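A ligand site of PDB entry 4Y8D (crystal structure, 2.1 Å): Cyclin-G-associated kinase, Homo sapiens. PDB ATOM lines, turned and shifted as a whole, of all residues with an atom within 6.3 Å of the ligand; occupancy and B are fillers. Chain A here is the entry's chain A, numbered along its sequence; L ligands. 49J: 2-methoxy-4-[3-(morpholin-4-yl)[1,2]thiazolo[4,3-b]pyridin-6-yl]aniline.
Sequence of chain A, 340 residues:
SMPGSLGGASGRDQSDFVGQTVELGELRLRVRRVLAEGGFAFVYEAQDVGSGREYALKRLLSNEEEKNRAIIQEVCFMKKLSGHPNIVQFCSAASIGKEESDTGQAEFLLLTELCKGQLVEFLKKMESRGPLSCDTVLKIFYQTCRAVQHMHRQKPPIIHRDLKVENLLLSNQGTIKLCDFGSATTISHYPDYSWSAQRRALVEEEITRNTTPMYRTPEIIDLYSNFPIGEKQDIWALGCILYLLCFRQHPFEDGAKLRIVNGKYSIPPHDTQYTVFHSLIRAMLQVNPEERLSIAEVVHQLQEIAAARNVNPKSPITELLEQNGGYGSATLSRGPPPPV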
ATOM      1  N   ARG A  33      -9.911   1.910  -5.062  1.00  0.00           N
ATOM      2  CA  ARG A  33     -11.068   1.661  -5.935  1.00  0.00           C
ATOM      3  C   ARG A  33     -10.716   0.837  -7.185  1.00  0.00           C
ATOM      4  O   ARG A  33      -9.543   0.624  -7.490  1.00  0.00           O
ATOM      5  CB  ARG A  33     -11.712   2.996  -6.364  1.00  0.00           C
ATOM      6  CG  ARG A  33     -10.714   4.067  -6.820  1.00  0.00           C
ATOM      7  CD  ARG A  33     -11.279   4.963  -7.904  1.00  0.00           C
ATOM      8  NE  ARG A  33     -10.318   5.992  -8.309  1.00  0.00           N
ATOM      9  CZ  ARG A  33     -10.421   6.741  -9.409  1.00  0.00           C
ATOM     10  NH1 ARG A  33     -11.452   6.618 -10.227  1.00  0.00           N
ATOM     11  NH2 ARG A  33      -9.471   7.635  -9.676  1.00  0.00           N
ATOM     12  N   LEU A  35     -10.604   0.392 -11.256  1.00  0.00           N
ATOM     13  CA  LEU A  35     -10.488   1.193 -12.487  1.00  0.00           C
ATOM     14  C   LEU A  35     -10.965   0.412 -13.722  1.00  0.00           C
ATOM     15  O   LEU A  35     -11.591   0.999 -14.607  1.00  0.00           O
ATOM     16  CB  LEU A  35      -9.044   1.667 -12.676  1.00  0.00           C
ATOM     17  CG  LEU A  35      -8.494   2.501 -11.514  1.00  0.00           C
ATOM     18  CD1 LEU A  35      -6.993   2.663 -11.607  1.00  0.00           C
ATOM     19  CD2 LEU A  35      -9.186   3.855 -11.480  1.00  0.00           C
ATOM     20  N   ALA A  36     -10.648  -0.888 -13.798  1.00  0.00           N
ATOM     21  CA  ALA A  36     -11.121  -1.770 -14.876  1.00  0.00           C
ATOM     22  C   ALA A  36     -11.232  -3.216 -14.388  1.00  0.00           C
ATOM     23  O   ALA A  36     -10.390  -3.660 -13.594  1.00  0.00           O
ATOM     24  CB  ALA A  36     -10.183  -1.696 -16.071  1.00  0.00           C
ATOM     25  N   VAL A  43      -7.849  -4.027 -12.389  1.00  0.00           N
ATOM     26  CA  VAL A  43      -6.954  -2.899 -12.145  1.00  0.00           C
ATOM     27  C   VAL A  43      -7.552  -1.969 -11.099  1.00  0.00           C
ATOM     28  O   VAL A  43      -8.741  -1.662 -11.158  1.00  0.00           O
ATOM     29  CB  VAL A  43      -6.676  -2.102 -13.448  1.00  0.00           C
ATOM     30  CG1 VAL A  43      -5.584  -1.060 -13.226  1.00  0.00           C
ATOM     31  CG2 VAL A  43      -6.303  -3.047 -14.572  1.00  0.00           C
ATOM     32  N   GLU A  45      -6.787   1.584  -8.264  1.00  0.00           N
ATOM     33  CA  GLU A  45      -5.986   2.700  -7.775  1.00  0.00           C
ATOM     34  C   GLU A  45      -5.439   2.320  -6.407  1.00  0.00           C
ATOM     35  O   GLU A  45      -6.170   1.768  -5.591  1.00  0.00           O
ATOM     36  CB  GLU A  45      -6.834   3.974  -7.664  1.00  0.00           C
ATOM     37  CG  GLU A  45      -6.055   5.229  -7.284  1.00  0.00           C
ATOM     38  CD  GLU A  45      -6.913   6.481  -7.251  1.00  0.00           C
ATOM     39  OE1 GLU A  45      -6.526   7.491  -7.882  1.00  0.00           O
ATOM     40  OE2 GLU A  45      -7.992   6.475  -6.609  1.00  0.00           O
ATOM     41  N   ALA A  56      -0.991   2.632 -10.038  1.00  0.00           N
ATOM     42  CA  ALA A  56      -1.883   1.636 -10.614  1.00  0.00           C
ATOM     43  C   ALA A  56      -1.430   0.254 -10.170  1.00  0.00           C
ATOM     44  O   ALA A  56      -0.223  -0.002  -9.991  1.00  0.00           O
ATOM     45  CB  ALA A  56      -1.896   1.720 -12.140  1.00  0.00           C
ATOM     46  N   LEU A  57      -2.406  -0.619  -9.944  1.00  0.00           N
ATOM     47  CA  LEU A  57      -2.119  -1.963  -9.450  1.00  0.00           C
ATOM     48  C   LEU A  57      -2.939  -2.949 -10.236  1.00  0.00           C
ATOM     49  O   LEU A  57      -4.175  -2.904 -10.183  1.00  0.00           O
ATOM     50  CB  LEU A  57      -2.425  -2.064  -7.954  1.00  0.00           C
ATOM     51  CG  LEU A  57      -2.215  -3.440  -7.304  1.00  0.00           C
ATOM     52  CD1 LEU A  57      -0.743  -3.783  -7.217  1.00  0.00           C
ATOM     53  CD2 LEU A  57      -2.815  -3.454  -5.924  1.00  0.00           C
ATOM     54  N   LYS A  58      -2.279  -3.815 -10.988  1.00  0.00           N
ATOM     55  CA  LYS A  58      -2.962  -4.836 -11.746  1.00  0.00           C
ATOM     56  C   LYS A  58      -2.825  -6.161 -11.008  1.00  0.00           C
ATOM     57  O   LYS A  58      -1.733  -6.538 -10.573  1.00  0.00           O
ATOM     58  CB  LYS A  58      -2.385  -4.973 -13.161  1.00  0.00           C
ATOM     59  CG  LYS A  58      -3.132  -5.947 -14.041  1.00  0.00           C
ATOM     60  CD  LYS A  58      -2.804  -5.686 -15.506  1.00  0.00           C
ATOM     61  CE  LYS A  58      -3.412  -6.724 -16.429  1.00  0.00           C
ATOM     62  NZ  LYS A  58      -2.830  -6.521 -17.793  1.00  0.00           N
ATOM     63  N   GLU A  74       4.421 -11.261 -19.189  1.00  0.00           N
ATOM     64  CA  GLU A  74       3.908  -9.904 -19.221  1.00  0.00           C
ATOM     65  C   GLU A  74       4.642  -8.969 -18.266  1.00  0.00           C
ATOM     66  O   GLU A  74       5.023  -7.850 -18.646  1.00  0.00           O
ATOM     67  CB  GLU A  74       2.405  -9.895 -18.916  1.00  0.00           C
ATOM     68  CG  GLU A  74       1.834  -8.514 -18.686  1.00  0.00           C
ATOM     69  CD  GLU A  74       0.316  -8.504 -18.593  1.00  0.00           C
ATOM     70  OE1 GLU A  74      -0.338  -9.568 -18.698  1.00  0.00           O
ATOM     71  OE2 GLU A  74      -0.218  -7.388 -18.416  1.00  0.00           O
ATOM     72  N   MET A  78       6.980  -5.714 -19.222  1.00  0.00           N
ATOM     73  CA  MET A  78       6.764  -4.420 -18.608  1.00  0.00           C
ATOM     74  C   MET A  78       8.060  -3.869 -18.021  1.00  0.00           C
ATOM     75  O   MET A  78       8.395  -2.710 -18.217  1.00  0.00           O
ATOM     76  CB  MET A  78       5.685  -4.534 -17.545  1.00  0.00           C
ATOM     77  CG  MET A  78       5.349  -3.227 -16.830  1.00  0.00           C
ATOM     78  SD  MET A  78       4.436  -2.053 -17.849  1.00  0.00           S
ATOM     79  CE  MET A  78       2.798  -2.787 -17.765  1.00  0.00           C
ATOM     80  N   VAL A  88       4.092   2.955 -19.982  1.00  0.00           N
ATOM     81  CA  VAL A  88       3.810   3.016 -18.533  1.00  0.00           C
ATOM     82  C   VAL A  88       5.043   2.565 -17.727  1.00  0.00           C
ATOM     83  O   VAL A  88       5.674   1.584 -18.059  1.00  0.00           O
ATOM     84  CB  VAL A  88       2.587   2.160 -18.073  1.00  0.00           C
ATOM     85  CG1 VAL A  88       1.293   2.620 -18.716  1.00  0.00           C
ATOM     86  CG2 VAL A  88       2.809   0.712 -18.389  1.00  0.00           C
ATOM     87  N   LEU A 110       1.103  -6.318 -10.099  1.00  0.00           N
ATOM     88  CA  LEU A 110       1.976  -5.481 -10.911  1.00  0.00           C
ATOM     89  C   LEU A 110       1.714  -4.032 -10.545  1.00  0.00           C
ATOM     90  O   LEU A 110       0.564  -3.569 -10.621  1.00  0.00           O
ATOM     91  CB  LEU A 110       1.707  -5.730 -12.388  1.00  0.00           C
ATOM     92  CG  LEU A 110       2.413  -4.822 -13.400  1.00  0.00           C
ATOM     93  CD1 LEU A 110       3.932  -5.007 -13.383  1.00  0.00           C
ATOM     94  CD2 LEU A 110       1.848  -5.048 -14.793  1.00  0.00           C
ATOM     95  N   THR A 112       2.465  -0.049 -11.219  1.00  0.00           N
ATOM     96  CA  THR A 112       2.964   0.919 -12.184  1.00  0.00           C
ATOM     97  C   THR A 112       2.622   2.341 -11.757  1.00  0.00           C
ATOM     98  O   THR A 112       1.853   2.545 -10.815  1.00  0.00           O
ATOM     99  CB  THR A 112       2.363   0.680 -13.590  1.00  0.00           C
ATOM    100  OG1 THR A 112       0.965   0.944 -13.586  1.00  0.00           O
ATOM    101  CG2 THR A 112       2.615  -0.757 -14.032  1.00  0.00           C
ATOM    102  N   GLU A 113       3.201   3.315 -12.448  1.00  0.00           N
ATOM    103  CA  GLU A 113       2.729   4.686 -12.328  1.00  0.00           C
ATOM    104  C   GLU A 113       1.256   4.711 -12.721  1.00  0.00           C
ATOM    105  O   GLU A 113       0.789   3.851 -13.495  1.00  0.00           O
ATOM    106  CB  GLU A 113       3.506   5.614 -13.244  1.00  0.00           C
ATOM    107  CG  GLU A 113       3.277   5.334 -14.739  1.00  0.00           C
ATOM    108  CD  GLU A 113       3.779   6.466 -15.626  1.00  0.00           C
ATOM    109  OE1 GLU A 113       3.832   7.604 -15.138  1.00  0.00           O
ATOM    110  OE2 GLU A 113       4.141   6.223 -16.802  1.00  0.00           O
ATOM    111  N   LEU A 114       0.529   5.649 -12.136  1.00  0.00           N
ATOM    112  CA  LEU A 114      -0.894   5.837 -12.394  1.00  0.00           C
ATOM    113  C   LEU A 114      -1.055   6.929 -13.428  1.00  0.00           C
ATOM    114  O   LEU A 114      -0.651   8.065 -13.198  1.00  0.00           O
ATOM    115  CB  LEU A 114      -1.595   6.242 -11.093  1.00  0.00           C
ATOM    116  CG  LEU A 114      -3.119   6.452 -11.154  1.00  0.00           C
ATOM    117  CD1 LEU A 114      -3.818   5.161 -11.532  1.00  0.00           C
ATOM    118  CD2 LEU A 114      -3.612   6.977  -9.803  1.00  0.00           C
ATOM    119  N   CYS A 115      -1.617   6.580 -14.579  1.00  0.00           N
ATOM    120  CA  CYS A 115      -1.958   7.563 -15.595  1.00  0.00           C
ATOM    121  C   CYS A 115      -3.271   8.246 -15.218  1.00  0.00           C
ATOM    122  O   CYS A 115      -3.964   7.815 -14.284  1.00  0.00           O
ATOM    123  CB  CYS A 115      -2.050   6.903 -16.961  1.00  0.00           C
ATOM    124  SG  CYS A 115      -0.514   6.045 -17.378  1.00  0.00           S
ATOM    125  N   LYS A 116      -3.593   9.301 -15.951  1.00  0.00           N
ATOM    126  CA  LYS A 116      -4.817  10.068 -15.717  1.00  0.00           C
ATOM    127  C   LYS A 116      -6.077   9.314 -16.171  1.00  0.00           C
ATOM    128  O   LYS A 116      -7.157   9.532 -15.629  1.00  0.00           O
ATOM    129  CB  LYS A 116      -4.703  11.398 -16.443  1.00  0.00           C
ATOM    130  CG  LYS A 116      -5.823  12.382 -16.190  1.00  0.00           C
ATOM    131  CD  LYS A 116      -5.627  13.629 -17.059  1.00  0.00           C
ATOM    132  CE  LYS A 116      -4.576  14.568 -16.494  1.00  0.00           C
ATOM    133  NZ  LYS A 116      -5.075  15.294 -15.296  1.00  0.00           N
ATOM    134  N   GLY A 117      -5.956   8.419 -17.141  1.00  0.00           N
ATOM    135  CA  GLY A 117      -7.101   7.680 -17.648  1.00  0.00           C
ATOM    136  C   GLY A 117      -6.921   7.198 -19.077  1.00  0.00           C
ATOM    137  O   GLY A 117      -5.824   7.246 -19.621  1.00  0.00           O
ATOM    138  N   GLN A 118      -8.006   6.764 -19.680  1.00  0.00           N
ATOM    139  CA  GLN A 118      -7.974   6.118 -20.970  1.00  0.00           C
ATOM    140  C   GLN A 118      -8.089   7.148 -22.101  1.00  0.00           C
ATOM    141  O   GLN A 118      -8.955   8.016 -22.062  1.00  0.00           O
ATOM    142  CB  GLN A 118      -9.096   5.105 -21.044  1.00  0.00           C
ATOM    143  CG  GLN A 118      -8.921   4.086 -22.135  1.00  0.00           C
ATOM    144  CD  GLN A 118      -9.685   2.812 -21.876  1.00  0.00           C
ATOM    145  OE1 GLN A 118      -9.715   2.308 -20.749  1.00  0.00           O
ATOM    146  NE2 GLN A 118     -10.335   2.281 -22.910  1.00  0.00           N
ATOM    147  N   LEU A 169      -3.212   5.022 -22.924  1.00  0.00           N
ATOM    148  CA  LEU A 169      -3.541   5.862 -21.783  1.00  0.00           C
ATOM    149  C   LEU A 169      -2.994   7.267 -21.977  1.00  0.00           C
ATOM    150  O   LEU A 169      -2.048   7.459 -22.713  1.00  0.00           O
ATOM    151  CB  LEU A 169      -2.939   5.251 -20.527  1.00  0.00           C
ATOM    152  CG  LEU A 169      -3.369   3.816 -20.224  1.00  0.00           C
ATOM    153  CD1 LEU A 169      -2.531   3.224 -19.081  1.00  0.00           C
ATOM    154  CD2 LEU A 169      -4.838   3.824 -19.858  1.00  0.00           C
ATOM    155  N   CYS A 179       0.400   0.482 -22.814  1.00  0.00           N
ATOM    156  CA  CYS A 179       0.434  -0.615 -21.860  1.00  0.00           C
ATOM    157  C   CYS A 179      -0.121  -1.868 -22.524  1.00  0.00           C
ATOM    158  O   CYS A 179      -0.189  -1.913 -23.764  1.00  0.00           O
ATOM    159  CB  CYS A 179      -0.379  -0.239 -20.625  1.00  0.00           C
ATOM    160  SG  CYS A 179      -2.139  -0.126 -20.994  1.00  0.00           S
ATOM    161  N   ASP A 180      -0.484  -2.886 -21.732  1.00  0.00           N
ATOM    162  CA  ASP A 180      -1.161  -4.080 -22.208  1.00  0.00           C
ATOM    163  C   ASP A 180      -0.176  -4.973 -22.961  1.00  0.00           C
ATOM    164  O   ASP A 180      -0.286  -5.180 -24.171  1.00  0.00           O
ATOM    165  CB  ASP A 180      -2.380  -3.719 -23.085  1.00  0.00           C
ATOM    166  CG  ASP A 180      -3.390  -4.861 -23.217  1.00  0.00           C
ATOM    167  OD1 ASP A 180      -3.025  -5.935 -23.748  1.00  0.00           O
ATOM    168  OD2 ASP A 180      -4.566  -4.675 -22.813  1.00  0.00           O
HETATM  169  CAJ 49J L   1      -0.798  -0.113 -15.746  1.00  0.00           C
HETATM  170  CAH 49J L   1      -0.653  -1.328 -16.428  1.00  0.00           C
HETATM  171  OAO 49J L   1      -1.554  -2.211 -15.743  1.00  0.00           O
HETATM  172  CAI 49J L   1      -2.932  -2.046 -16.167  1.00  0.00           C
HETATM  173  CAK 49J L   1      -3.134  -0.615 -16.738  1.00  0.00           C
HETATM  174  NAX 49J L   1      -2.163   0.347 -16.126  1.00  0.00           N
HETATM  175  CAU 49J L   1      -2.477   1.603 -15.830  1.00  0.00           C
HETATM  176  SAP 49J L   1      -1.429   2.635 -15.443  1.00  0.00           S
HETATM  177  NAM 49J L   1      -2.420   3.888 -15.164  1.00  0.00           N
HETATM  178  CAV 49J L   1      -3.654   3.436 -15.397  1.00  0.00           C
HETATM  179  CAG 49J L   1      -4.795   4.126 -15.319  1.00  0.00           C
HETATM  180  CAW 49J L   1      -3.691   2.146 -15.777  1.00  0.00           C
HETATM  181  NAL 49J L   1      -4.862   1.568 -16.058  1.00  0.00           N
HETATM  182  CAE 49J L   1      -6.058   2.257 -15.982  1.00  0.00           C
HETATM  183  CAS 49J L   1      -6.038   3.579 -15.620  1.00  0.00           C
HETATM  184  CAR 49J L   1      -7.230   4.300 -15.494  1.00  0.00           C
HETATM  185  CAF 49J L   1      -7.329   5.360 -14.563  1.00  0.00           C
HETATM  186  CAD 49J L   1      -8.341   3.939 -16.257  1.00  0.00           C
HETATM  187  CAC 49J L   1      -9.549   4.628 -16.118  1.00  0.00           C
HETATM  188  CAQ 49J L   1      -9.632   5.663 -15.206  1.00  0.00           C
HETATM  189  NAB 49J L   1     -10.763   6.342 -15.051  1.00  0.00           N
HETATM  190  CAT 49J L   1      -8.535   6.040 -14.420  1.00  0.00           C
HETATM  191  OAN 49J L   1      -8.763   7.089 -13.557  1.00  0.00           O
HETATM  192  CAA 49J L   1      -7.591   7.726 -12.961  1.00  0.00           C
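NAM of the ligand lies within hydrogen-bond range of N of Cys 115, 2.9 Å away. A nitrogen (NAM) of the ligand sits close to the side-chain sulfur of Cys 115 (3.6 Å). SAP of the ligand lies close to OG1 of Thr 112 (3.5 Å).
O of Thr 112 is in hydrogen-bond range of N of Ala 56 (2.9 Å). O of Leu 110 sits at hydrogen-bond distance from N of Lys 58, at 2.9 Å. OE2 of Glu 74 is in salt-bridge range of NZ of Lys 58 (2.8 Å). N of Leu 35 is in hydrogen-bond range of O of Val 43, 2.8 Å away. OE2 of Glu 45 is in salt-bridge range of NE of Arg 33 (2.9 Å). O of Ala 36 lies within hydrogen-bond range of N of Val 43.
O of Glu 113 sits close to SAP of the ligand (3.2 Å). Arg 33 touches the ligand (NH2 to CAA, 3.8 Å). CD2 of Leu 35 touches CAT of the ligand, at 3.7 Å. Val 43 touches the ligand. Ala 56 touches the ligand. Lys 58 touches the ligand. Met 78 touches the ligand. Leu 114 touches the ligand. Lys 116 touches the ligand. Gly 117 touches the ligand. Leu 169 touches the ligand. Of the 22 residues printed, 13 come within 4 Å of the ligand.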
